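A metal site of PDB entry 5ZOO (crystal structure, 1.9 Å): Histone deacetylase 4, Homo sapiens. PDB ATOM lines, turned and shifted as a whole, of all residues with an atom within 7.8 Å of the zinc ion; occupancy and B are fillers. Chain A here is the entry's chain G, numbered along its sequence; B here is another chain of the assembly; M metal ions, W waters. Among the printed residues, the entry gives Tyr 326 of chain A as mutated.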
ATOM      1  N   ARG A  31       3.958  28.652  -8.648  1.00  0.00           N
ATOM      2  CA  ARG A  31       4.031  27.408  -7.877  1.00  0.00           C
ATOM      3  C   ARG A  31       3.551  26.214  -8.698  1.00  0.00           C
ATOM      4  O   ARG A  31       4.281  25.226  -8.854  1.00  0.00           O
ATOM      5  CB  ARG A  31       3.203  27.536  -6.590  1.00  0.00           C
ATOM      6  CG  ARG A  31       3.709  28.551  -5.568  1.00  0.00           C
ATOM      7  CD  ARG A  31       2.764  28.646  -4.367  1.00  0.00           C
ATOM      8  NE  ARG A  31       2.669  27.374  -3.659  1.00  0.00           N
ATOM      9  CZ  ARG A  31       1.571  26.624  -3.568  1.00  0.00           C
ATOM     10  NH1 ARG A  31       0.431  27.029  -4.130  1.00  0.00           N
ATOM     11  NH2 ARG A  31       1.605  25.473  -2.908  1.00  0.00           N
ATOM     12  N   PRO A 150      -4.610  26.830  -2.275  1.00  0.00           N
ATOM     13  CA  PRO A 150      -4.735  25.687  -1.365  1.00  0.00           C
ATOM     14  C   PRO A 150      -6.046  25.745  -0.595  1.00  0.00           C
ATOM     15  O   PRO A 150      -6.786  26.725  -0.720  1.00  0.00           O
ATOM     16  CB  PRO A 150      -3.516  25.842  -0.433  1.00  0.00           C
ATOM     17  CG  PRO A 150      -3.216  27.321  -0.454  1.00  0.00           C
ATOM     18  CD  PRO A 150      -3.540  27.755  -1.871  1.00  0.00           C
ATOM     19  N   HIS A 152      -6.769  23.760   2.932  1.00  0.00           N
ATOM     20  CA  HIS A 152      -7.039  23.140   4.236  1.00  0.00           C
ATOM     21  C   HIS A 152      -7.189  24.137   5.393  1.00  0.00           C
ATOM     22  O   HIS A 152      -7.592  23.717   6.477  1.00  0.00           O
ATOM     23  CB  HIS A 152      -5.977  22.072   4.563  1.00  0.00           C
ATOM     24  CG  HIS A 152      -4.611  22.629   4.826  1.00  0.00           C
ATOM     25  ND1 HIS A 152      -3.679  21.963   5.601  1.00  0.00           N
ATOM     26  CD2 HIS A 152      -4.008  23.770   4.416  1.00  0.00           C
ATOM     27  CE1 HIS A 152      -2.568  22.685   5.664  1.00  0.00           C
ATOM     28  NE2 HIS A 152      -2.737  23.778   4.950  1.00  0.00           N
ATOM     29  N   HIS A 153      -6.913  25.435   5.200  1.00  0.00           N
ATOM     30  CA  HIS A 153      -7.167  26.417   6.252  1.00  0.00           C
ATOM     31  C   HIS A 153      -8.555  27.048   6.167  1.00  0.00           C
ATOM     32  O   HIS A 153      -8.955  27.741   7.111  1.00  0.00           O
ATOM     33  CB  HIS A 153      -6.130  27.555   6.223  1.00  0.00           C
ATOM     34  CG  HIS A 153      -4.725  27.128   6.524  1.00  0.00           C
ATOM     35  ND1 HIS A 153      -4.384  26.393   7.641  1.00  0.00           N
ATOM     36  CD2 HIS A 153      -3.572  27.337   5.839  1.00  0.00           C
ATOM     37  CE1 HIS A 153      -3.085  26.167   7.624  1.00  0.00           C
ATOM     38  NE2 HIS A 153      -2.563  26.724   6.549  1.00  0.00           N
ATOM     39  N   GLY A 161      -5.242  32.106   5.480  1.00  0.00           N
ATOM     40  CA  GLY A 161      -4.024  31.357   5.178  1.00  0.00           C
ATOM     41  C   GLY A 161      -3.903  30.935   3.729  1.00  0.00           C
ATOM     42  O   GLY A 161      -3.486  29.812   3.443  1.00  0.00           O
ATOM     43  N   PHE A 162      -4.270  31.834   2.811  1.00  0.00           N
ATOM     44  CA  PHE A 162      -4.270  31.650   1.348  1.00  0.00           C
ATOM     45  C   PHE A 162      -5.446  30.797   0.846  1.00  0.00           C
ATOM     46  O   PHE A 162      -5.536  30.582  -0.377  1.00  0.00           O
ATOM     47  CB  PHE A 162      -2.984  31.003   0.798  1.00  0.00           C
ATOM     48  CG  PHE A 162      -1.699  31.673   1.249  1.00  0.00           C
ATOM     49  CD1 PHE A 162      -1.581  33.054   1.263  1.00  0.00           C
ATOM     50  CD2 PHE A 162      -0.614  30.898   1.626  1.00  0.00           C
ATOM     51  CE1 PHE A 162      -0.397  33.657   1.665  1.00  0.00           C
ATOM     52  CE2 PHE A 162       0.572  31.486   2.021  1.00  0.00           C
ATOM     53  CZ  PHE A 162       0.688  32.875   2.030  1.00  0.00           C
ATOM     54  N   CYS A 163      -6.340  30.319   1.717  1.00  0.00           N
ATOM     55  CA  CYS A 163      -7.361  29.344   1.341  1.00  0.00           C
ATOM     56  C   CYS A 163      -8.749  29.952   1.342  1.00  0.00           C
ATOM     57  O   CYS A 163      -9.098  30.720   2.234  1.00  0.00           O
ATOM     58  CB  CYS A 163      -7.350  28.150   2.304  1.00  0.00           C
ATOM     59  SG  CYS A 163      -5.750  27.322   2.476  1.00  0.00           S
ATOM     60  N   ASP A 188      -2.512  14.928   6.440  1.00  0.00           N
ATOM     61  CA  ASP A 188      -2.197  16.319   6.110  1.00  0.00           C
ATOM     62  C   ASP A 188      -0.748  16.545   6.523  1.00  0.00           C
ATOM     63  O   ASP A 188      -0.478  16.757   7.704  1.00  0.00           O
ATOM     64  CB  ASP A 188      -3.183  17.251   6.826  1.00  0.00           C
ATOM     65  CG  ASP A 188      -2.991  18.719   6.478  1.00  0.00           C
ATOM     66  OD1 ASP A 188      -1.853  19.132   6.156  1.00  0.00           O
ATOM     67  OD2 ASP A 188      -3.992  19.473   6.536  1.00  0.00           O
ATOM     68  N   TRP A 189       0.192  16.477   5.584  1.00  0.00           N
ATOM     69  CA  TRP A 189       1.604  16.663   5.930  1.00  0.00           C
ATOM     70  C   TRP A 189       2.154  18.015   5.480  1.00  0.00           C
ATOM     71  O   TRP A 189       3.372  18.234   5.549  1.00  0.00           O
ATOM     72  CB  TRP A 189       2.469  15.505   5.388  1.00  0.00           C
ATOM     73  CG  TRP A 189       2.565  15.324   3.889  1.00  0.00           C
ATOM     74  CD1 TRP A 189       2.653  16.302   2.928  1.00  0.00           C
ATOM     75  CD2 TRP A 189       2.631  14.073   3.192  1.00  0.00           C
ATOM     76  NE1 TRP A 189       2.755  15.728   1.673  1.00  0.00           N
ATOM     77  CE2 TRP A 189       2.734  14.364   1.811  1.00  0.00           C
ATOM     78  CE3 TRP A 189       2.598  12.737   3.600  1.00  0.00           C
ATOM     79  CZ2 TRP A 189       2.818  13.353   0.843  1.00  0.00           C
ATOM     80  CZ3 TRP A 189       2.686  11.747   2.645  1.00  0.00           C
ATOM     81  CH2 TRP A 189       2.786  12.061   1.283  1.00  0.00           C
ATOM     82  N   ASP A 190       1.291  18.922   5.056  1.00  0.00           N
ATOM     83  CA  ASP A 190       1.650  20.334   5.048  1.00  0.00           C
ATOM     84  C   ASP A 190       2.168  20.720   6.428  1.00  0.00           C
ATOM     85  O   ASP A 190       1.726  20.186   7.447  1.00  0.00           O
ATOM     86  CB  ASP A 190       0.416  21.156   4.662  1.00  0.00           C
ATOM     87  CG  ASP A 190       0.716  22.630   4.505  1.00  0.00           C
ATOM     88  OD1 ASP A 190       0.942  23.295   5.530  1.00  0.00           O
ATOM     89  OD2 ASP A 190       0.723  23.111   3.350  1.00  0.00           O
ATOM     90  N   VAL A 191       3.150  21.623   6.470  1.00  0.00           N
ATOM     91  CA  VAL A 191       3.780  21.943   7.747  1.00  0.00           C
ATOM     92  C   VAL A 191       2.820  22.667   8.698  1.00  0.00           C
ATOM     93  O   VAL A 191       3.091  22.762   9.907  1.00  0.00           O
ATOM     94  CB  VAL A 191       5.054  22.787   7.534  1.00  0.00           C
ATOM     95  CG1 VAL A 191       4.706  24.258   7.257  1.00  0.00           C
ATOM     96  CG2 VAL A 191       5.990  22.655   8.726  1.00  0.00           C
ATOM     97  N   HIS A 192       1.716  23.185   8.183  1.00  0.00           N
ATOM     98  CA  HIS A 192       0.715  23.878   8.981  1.00  0.00           C
ATOM     99  C   HIS A 192      -0.450  22.960   9.310  1.00  0.00           C
ATOM    100  O   HIS A 192      -0.823  22.090   8.512  1.00  0.00           O
ATOM    101  CB  HIS A 192       0.168  25.101   8.238  1.00  0.00           C
ATOM    102  CG  HIS A 192       1.218  26.101   7.854  1.00  0.00           C
ATOM    103  ND1 HIS A 192       1.753  26.152   6.590  1.00  0.00           N
ATOM    104  CD2 HIS A 192       1.840  27.068   8.568  1.00  0.00           C
ATOM    105  CE1 HIS A 192       2.656  27.114   6.534  1.00  0.00           C
ATOM    106  NE2 HIS A 192       2.728  27.693   7.726  1.00  0.00           N
ATOM    107  N   HIS A 193      -1.053  23.170  10.481  1.00  0.00           N
ATOM    108  CA  HIS A 193      -2.261  22.431  10.853  1.00  0.00           C
ATOM    109  C   HIS A 193      -3.420  22.772   9.919  1.00  0.00           C
ATOM    110  O   HIS A 193      -3.677  23.941   9.628  1.00  0.00           O
ATOM    111  CB  HIS A 193      -2.638  22.752  12.299  1.00  0.00           C
ATOM    112  CG  HIS A 193      -3.882  22.065  12.765  1.00  0.00           C
ATOM    113  ND1 HIS A 193      -4.997  22.742  13.189  1.00  0.00           N
ATOM    114  CD2 HIS A 193      -4.172  20.743  12.883  1.00  0.00           C
ATOM    115  CE1 HIS A 193      -5.931  21.872  13.552  1.00  0.00           C
ATOM    116  NE2 HIS A 193      -5.453  20.651  13.372  1.00  0.00           N
ATOM    117  N   PHE A 220       2.568  29.067  16.311  1.00  0.00           N
ATOM    118  CA  PHE A 220       2.831  29.053  14.884  1.00  0.00           C
ATOM    119  C   PHE A 220       1.490  29.089  14.154  1.00  0.00           C
ATOM    120  O   PHE A 220       0.460  28.710  14.716  1.00  0.00           O
ATOM    121  CB  PHE A 220       3.659  27.816  14.503  1.00  0.00           C
ATOM    122  CG  PHE A 220       4.186  27.827  13.091  1.00  0.00           C
ATOM    123  CD1 PHE A 220       5.128  28.776  12.690  1.00  0.00           C
ATOM    124  CD2 PHE A 220       3.771  26.874  12.178  1.00  0.00           C
ATOM    125  CE1 PHE A 220       5.619  28.781  11.396  1.00  0.00           C
ATOM    126  CE2 PHE A 220       4.255  26.866  10.867  1.00  0.00           C
ATOM    127  CZ  PHE A 220       5.180  27.827  10.476  1.00  0.00           C
ATOM    128  N   PHE A 221       1.494  29.551  12.904  1.00  0.00           N
ATOM    129  CA  PHE A 221       0.240  29.637  12.161  1.00  0.00           C
ATOM    130  C   PHE A 221      -0.306  28.234  11.887  1.00  0.00           C
ATOM    131  O   PHE A 221       0.451  27.337  11.490  1.00  0.00           O
ATOM    132  CB  PHE A 221       0.429  30.373  10.839  1.00  0.00           C
ATOM    133  CG  PHE A 221      -0.858  30.599  10.088  1.00  0.00           C
ATOM    134  CD1 PHE A 221      -1.625  31.720  10.331  1.00  0.00           C
ATOM    135  CD2 PHE A 221      -1.330  29.661   9.176  1.00  0.00           C
ATOM    136  CE1 PHE A 221      -2.826  31.930   9.662  1.00  0.00           C
ATOM    137  CE2 PHE A 221      -2.527  29.855   8.499  1.00  0.00           C
ATOM    138  CZ  PHE A 221      -3.277  31.001   8.752  1.00  0.00           C
ATOM    139  N   GLY A 282       0.934  19.471   1.258  1.00  0.00           N
ATOM    140  CA  GLY A 282       1.775  20.646   1.234  1.00  0.00           C
ATOM    141  C   GLY A 282       3.234  20.258   1.357  1.00  0.00           C
ATOM    142  O   GLY A 282       3.571  19.225   1.936  1.00  0.00           O
ATOM    143  N   PHE A 283       4.110  21.073   0.790  1.00  0.00           N
ATOM    144  CA  PHE A 283       5.541  20.797   0.807  1.00  0.00           C
ATOM    145  C   PHE A 283       6.342  21.892   1.517  1.00  0.00           C
ATOM    146  O   PHE A 283       7.548  22.022   1.294  1.00  0.00           O
ATOM    147  CB  PHE A 283       6.064  20.598  -0.630  1.00  0.00           C
ATOM    148  CG  PHE A 283       5.507  19.372  -1.308  1.00  0.00           C
ATOM    149  CD1 PHE A 283       5.540  18.126  -0.683  1.00  0.00           C
ATOM    150  CD2 PHE A 283       4.943  19.458  -2.577  1.00  0.00           C
ATOM    151  CE1 PHE A 283       5.032  16.996  -1.312  1.00  0.00           C
ATOM    152  CE2 PHE A 283       4.418  18.332  -3.208  1.00  0.00           C
ATOM    153  CZ  PHE A 283       4.468  17.089  -2.568  1.00  0.00           C
ATOM    154  N   ASP A 284       5.693  22.659   2.398  1.00  0.00           N
ATOM    155  CA  ASP A 284       6.413  23.702   3.115  1.00  0.00           C
ATOM    156  C   ASP A 284       7.212  23.175   4.326  1.00  0.00           C
ATOM    157  O   ASP A 284       7.783  23.986   5.057  1.00  0.00           O
ATOM    158  CB  ASP A 284       5.457  24.827   3.554  1.00  0.00           C
ATOM    159  CG  ASP A 284       4.060  24.328   3.921  1.00  0.00           C
ATOM    160  OD1 ASP A 284       3.866  23.118   4.128  1.00  0.00           O
ATOM    161  OD2 ASP A 284       3.155  25.188   4.015  1.00  0.00           O
ATOM    162  N   ALA A 285       7.272  21.861   4.540  1.00  0.00           N
ATOM    163  CA  ALA A 285       8.219  21.276   5.488  1.00  0.00           C
ATOM    164  C   ALA A 285       9.536  20.893   4.825  1.00  0.00           C
ATOM    165  O   ALA A 285      10.463  20.463   5.528  1.00  0.00           O
ATOM    166  CB  ALA A 285       7.608  20.053   6.183  1.00  0.00           C
ATOM    167  N   LEU A 293       7.730  30.437   7.190  1.00  0.00           N
ATOM    168  CA  LEU A 293       6.776  29.676   6.403  1.00  0.00           C
ATOM    169  C   LEU A 293       6.826  28.182   6.689  1.00  0.00           C
ATOM    170  O   LEU A 293       5.970  27.442   6.191  1.00  0.00           O
ATOM    171  CB  LEU A 293       7.021  29.895   4.906  1.00  0.00           C
ATOM    172  CG  LEU A 293       6.587  31.233   4.307  1.00  0.00           C
ATOM    173  CD1 LEU A 293       7.002  31.318   2.845  1.00  0.00           C
ATOM    174  CD2 LEU A 293       5.077  31.382   4.439  1.00  0.00           C
ATOM    175  N   GLY A 294       7.795  27.725   7.465  1.00  0.00           N
ATOM    176  CA  GLY A 294       7.891  26.312   7.801  1.00  0.00           C
ATOM    177  C   GLY A 294       9.131  26.061   8.625  1.00  0.00           C
ATOM    178  O   GLY A 294       9.052  25.810   9.827  1.00  0.00           O
ATOM    179  N   GLU A 323      -1.212  21.426  -1.262  1.00  0.00           N
ATOM    180  CA  GLU A 323      -1.641  22.530  -0.408  1.00  0.00           C
ATOM    181  C   GLU A 323      -0.585  23.627  -0.480  1.00  0.00           C
ATOM    182  O   GLU A 323      -0.450  24.285  -1.519  1.00  0.00           O
ATOM    183  CB  GLU A 323      -1.864  22.043   1.031  1.00  0.00           C
ATOM    184  CG  GLU A 323      -2.940  20.950   1.165  1.00  0.00           C
ATOM    185  CD  GLU A 323      -4.373  21.483   1.130  1.00  0.00           C
ATOM    186  OE1 GLU A 323      -5.326  20.680   1.241  1.00  0.00           O
ATOM    187  OE2 GLU A 323      -4.558  22.718   1.012  1.00  0.00           O
ATOM    188  N   GLY A 324       0.188  23.810   0.589  1.00  0.00           N
ATOM    189  CA  GLY A 324       1.242  24.803   0.634  1.00  0.00           C
ATOM    190  C   GLY A 324       2.571  24.284   0.108  1.00  0.00           C
ATOM    191  O   GLY A 324       2.655  23.239  -0.538  1.00  0.00           O
ATOM    192  N   GLY A 325       3.634  25.022   0.424  1.00  0.00           N
ATOM    193  CA  GLY A 325       4.938  24.803  -0.178  1.00  0.00           C
ATOM    194  C   GLY A 325       5.246  25.927  -1.138  1.00  0.00           C
ATOM    195  O   GLY A 325       4.482  26.163  -2.074  1.00  0.00           O
ATOM    196  N   TYR A 326       6.357  26.632  -0.933  1.00  0.00           N
ATOM    197  CA  TYR A 326       6.509  27.932  -1.568  1.00  0.00           C
ATOM    198  C   TYR A 326       7.828  28.076  -2.308  1.00  0.00           C
ATOM    199  O   TYR A 326       7.879  28.735  -3.354  1.00  0.00           O
ATOM    200  CB  TYR A 326       6.304  29.032  -0.511  1.00  0.00           C
ATOM    201  CG  TYR A 326       4.948  28.848   0.122  1.00  0.00           C
ATOM    202  CD1 TYR A 326       3.811  29.246  -0.559  1.00  0.00           C
ATOM    203  CD2 TYR A 326       4.798  28.206   1.348  1.00  0.00           C
ATOM    204  CE1 TYR A 326       2.558  29.051  -0.036  1.00  0.00           C
ATOM    205  CE2 TYR A 326       3.541  28.004   1.883  1.00  0.00           C
ATOM    206  CZ  TYR A 326       2.425  28.426   1.188  1.00  0.00           C
ATOM    207  OH  TYR A 326       1.169  28.254   1.690  1.00  0.00           O
ATOM    208  N   ILE B   6      -0.057  33.788   7.987  1.00  0.00           N
ATOM    209  CA  ILE B   6       0.715  32.632   7.552  1.00  0.00           C
ATOM    210  C   ILE B   6       2.050  33.077   6.964  1.00  0.00           C
ATOM    211  O   ILE B   6       3.059  32.383   7.132  1.00  0.00           O
ATOM    212  CB  ILE B   6      -0.102  31.764   6.571  1.00  0.00           C
ATOM    213  CG1 ILE B   6       0.647  30.465   6.244  1.00  0.00           C
ATOM    214  CG2 ILE B   6      -0.446  32.538   5.293  1.00  0.00           C
ATOM    215  CD1 ILE B   6      -0.199  29.441   5.476  1.00  0.00           C
HETATM  216 ZN    ZN M   1       1.279  25.169   4.756  1.00  0.00          ZN
HETATM  217  O   HOH W   1       0.676  26.657   3.328  1.00  0.00           O
HETATM  218  O   HOH W   2      -0.899  25.630   4.609  1.00  0.00           O
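The backbone NH (N) of Val 191 is in hydrogen-bond range of the side-chain carboxylate (OD1) of Asp 284 (2.9 Å).
N of Gly 324 lies close to OD2 of Asp 190.
The backbone NH (N) of Asp 190 lies within hydrogen-bond range of the side-chain carboxylate (OD1) of Asp 188 (3.3 Å).
Within 4 Å of the zinc ion: Asp 190, His 192 and Asp 284.
OD2 of Asp 284 binds the zinc ion (2.0 Å).
The side-chain carboxylate (OD1) of Asp 190 binds the zinc ion, 2.1 Å away.
ND1 of His 192 binds the zinc ion, at 2.1 Å.
Water W1 binds the zinc ion, at 2.1 Å.
The zinc ion is bound by water W2 (2.2 Å).
The side-chain carboxylate (OD2) of Asp 190 binds the zinc ion (2.6 Å).
The zinc ion has six donor atoms within binding distance.
Water W2 bridges a ring nitrogen (NE2) of His 152 and a ring nitrogen (NE2) of His 153.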
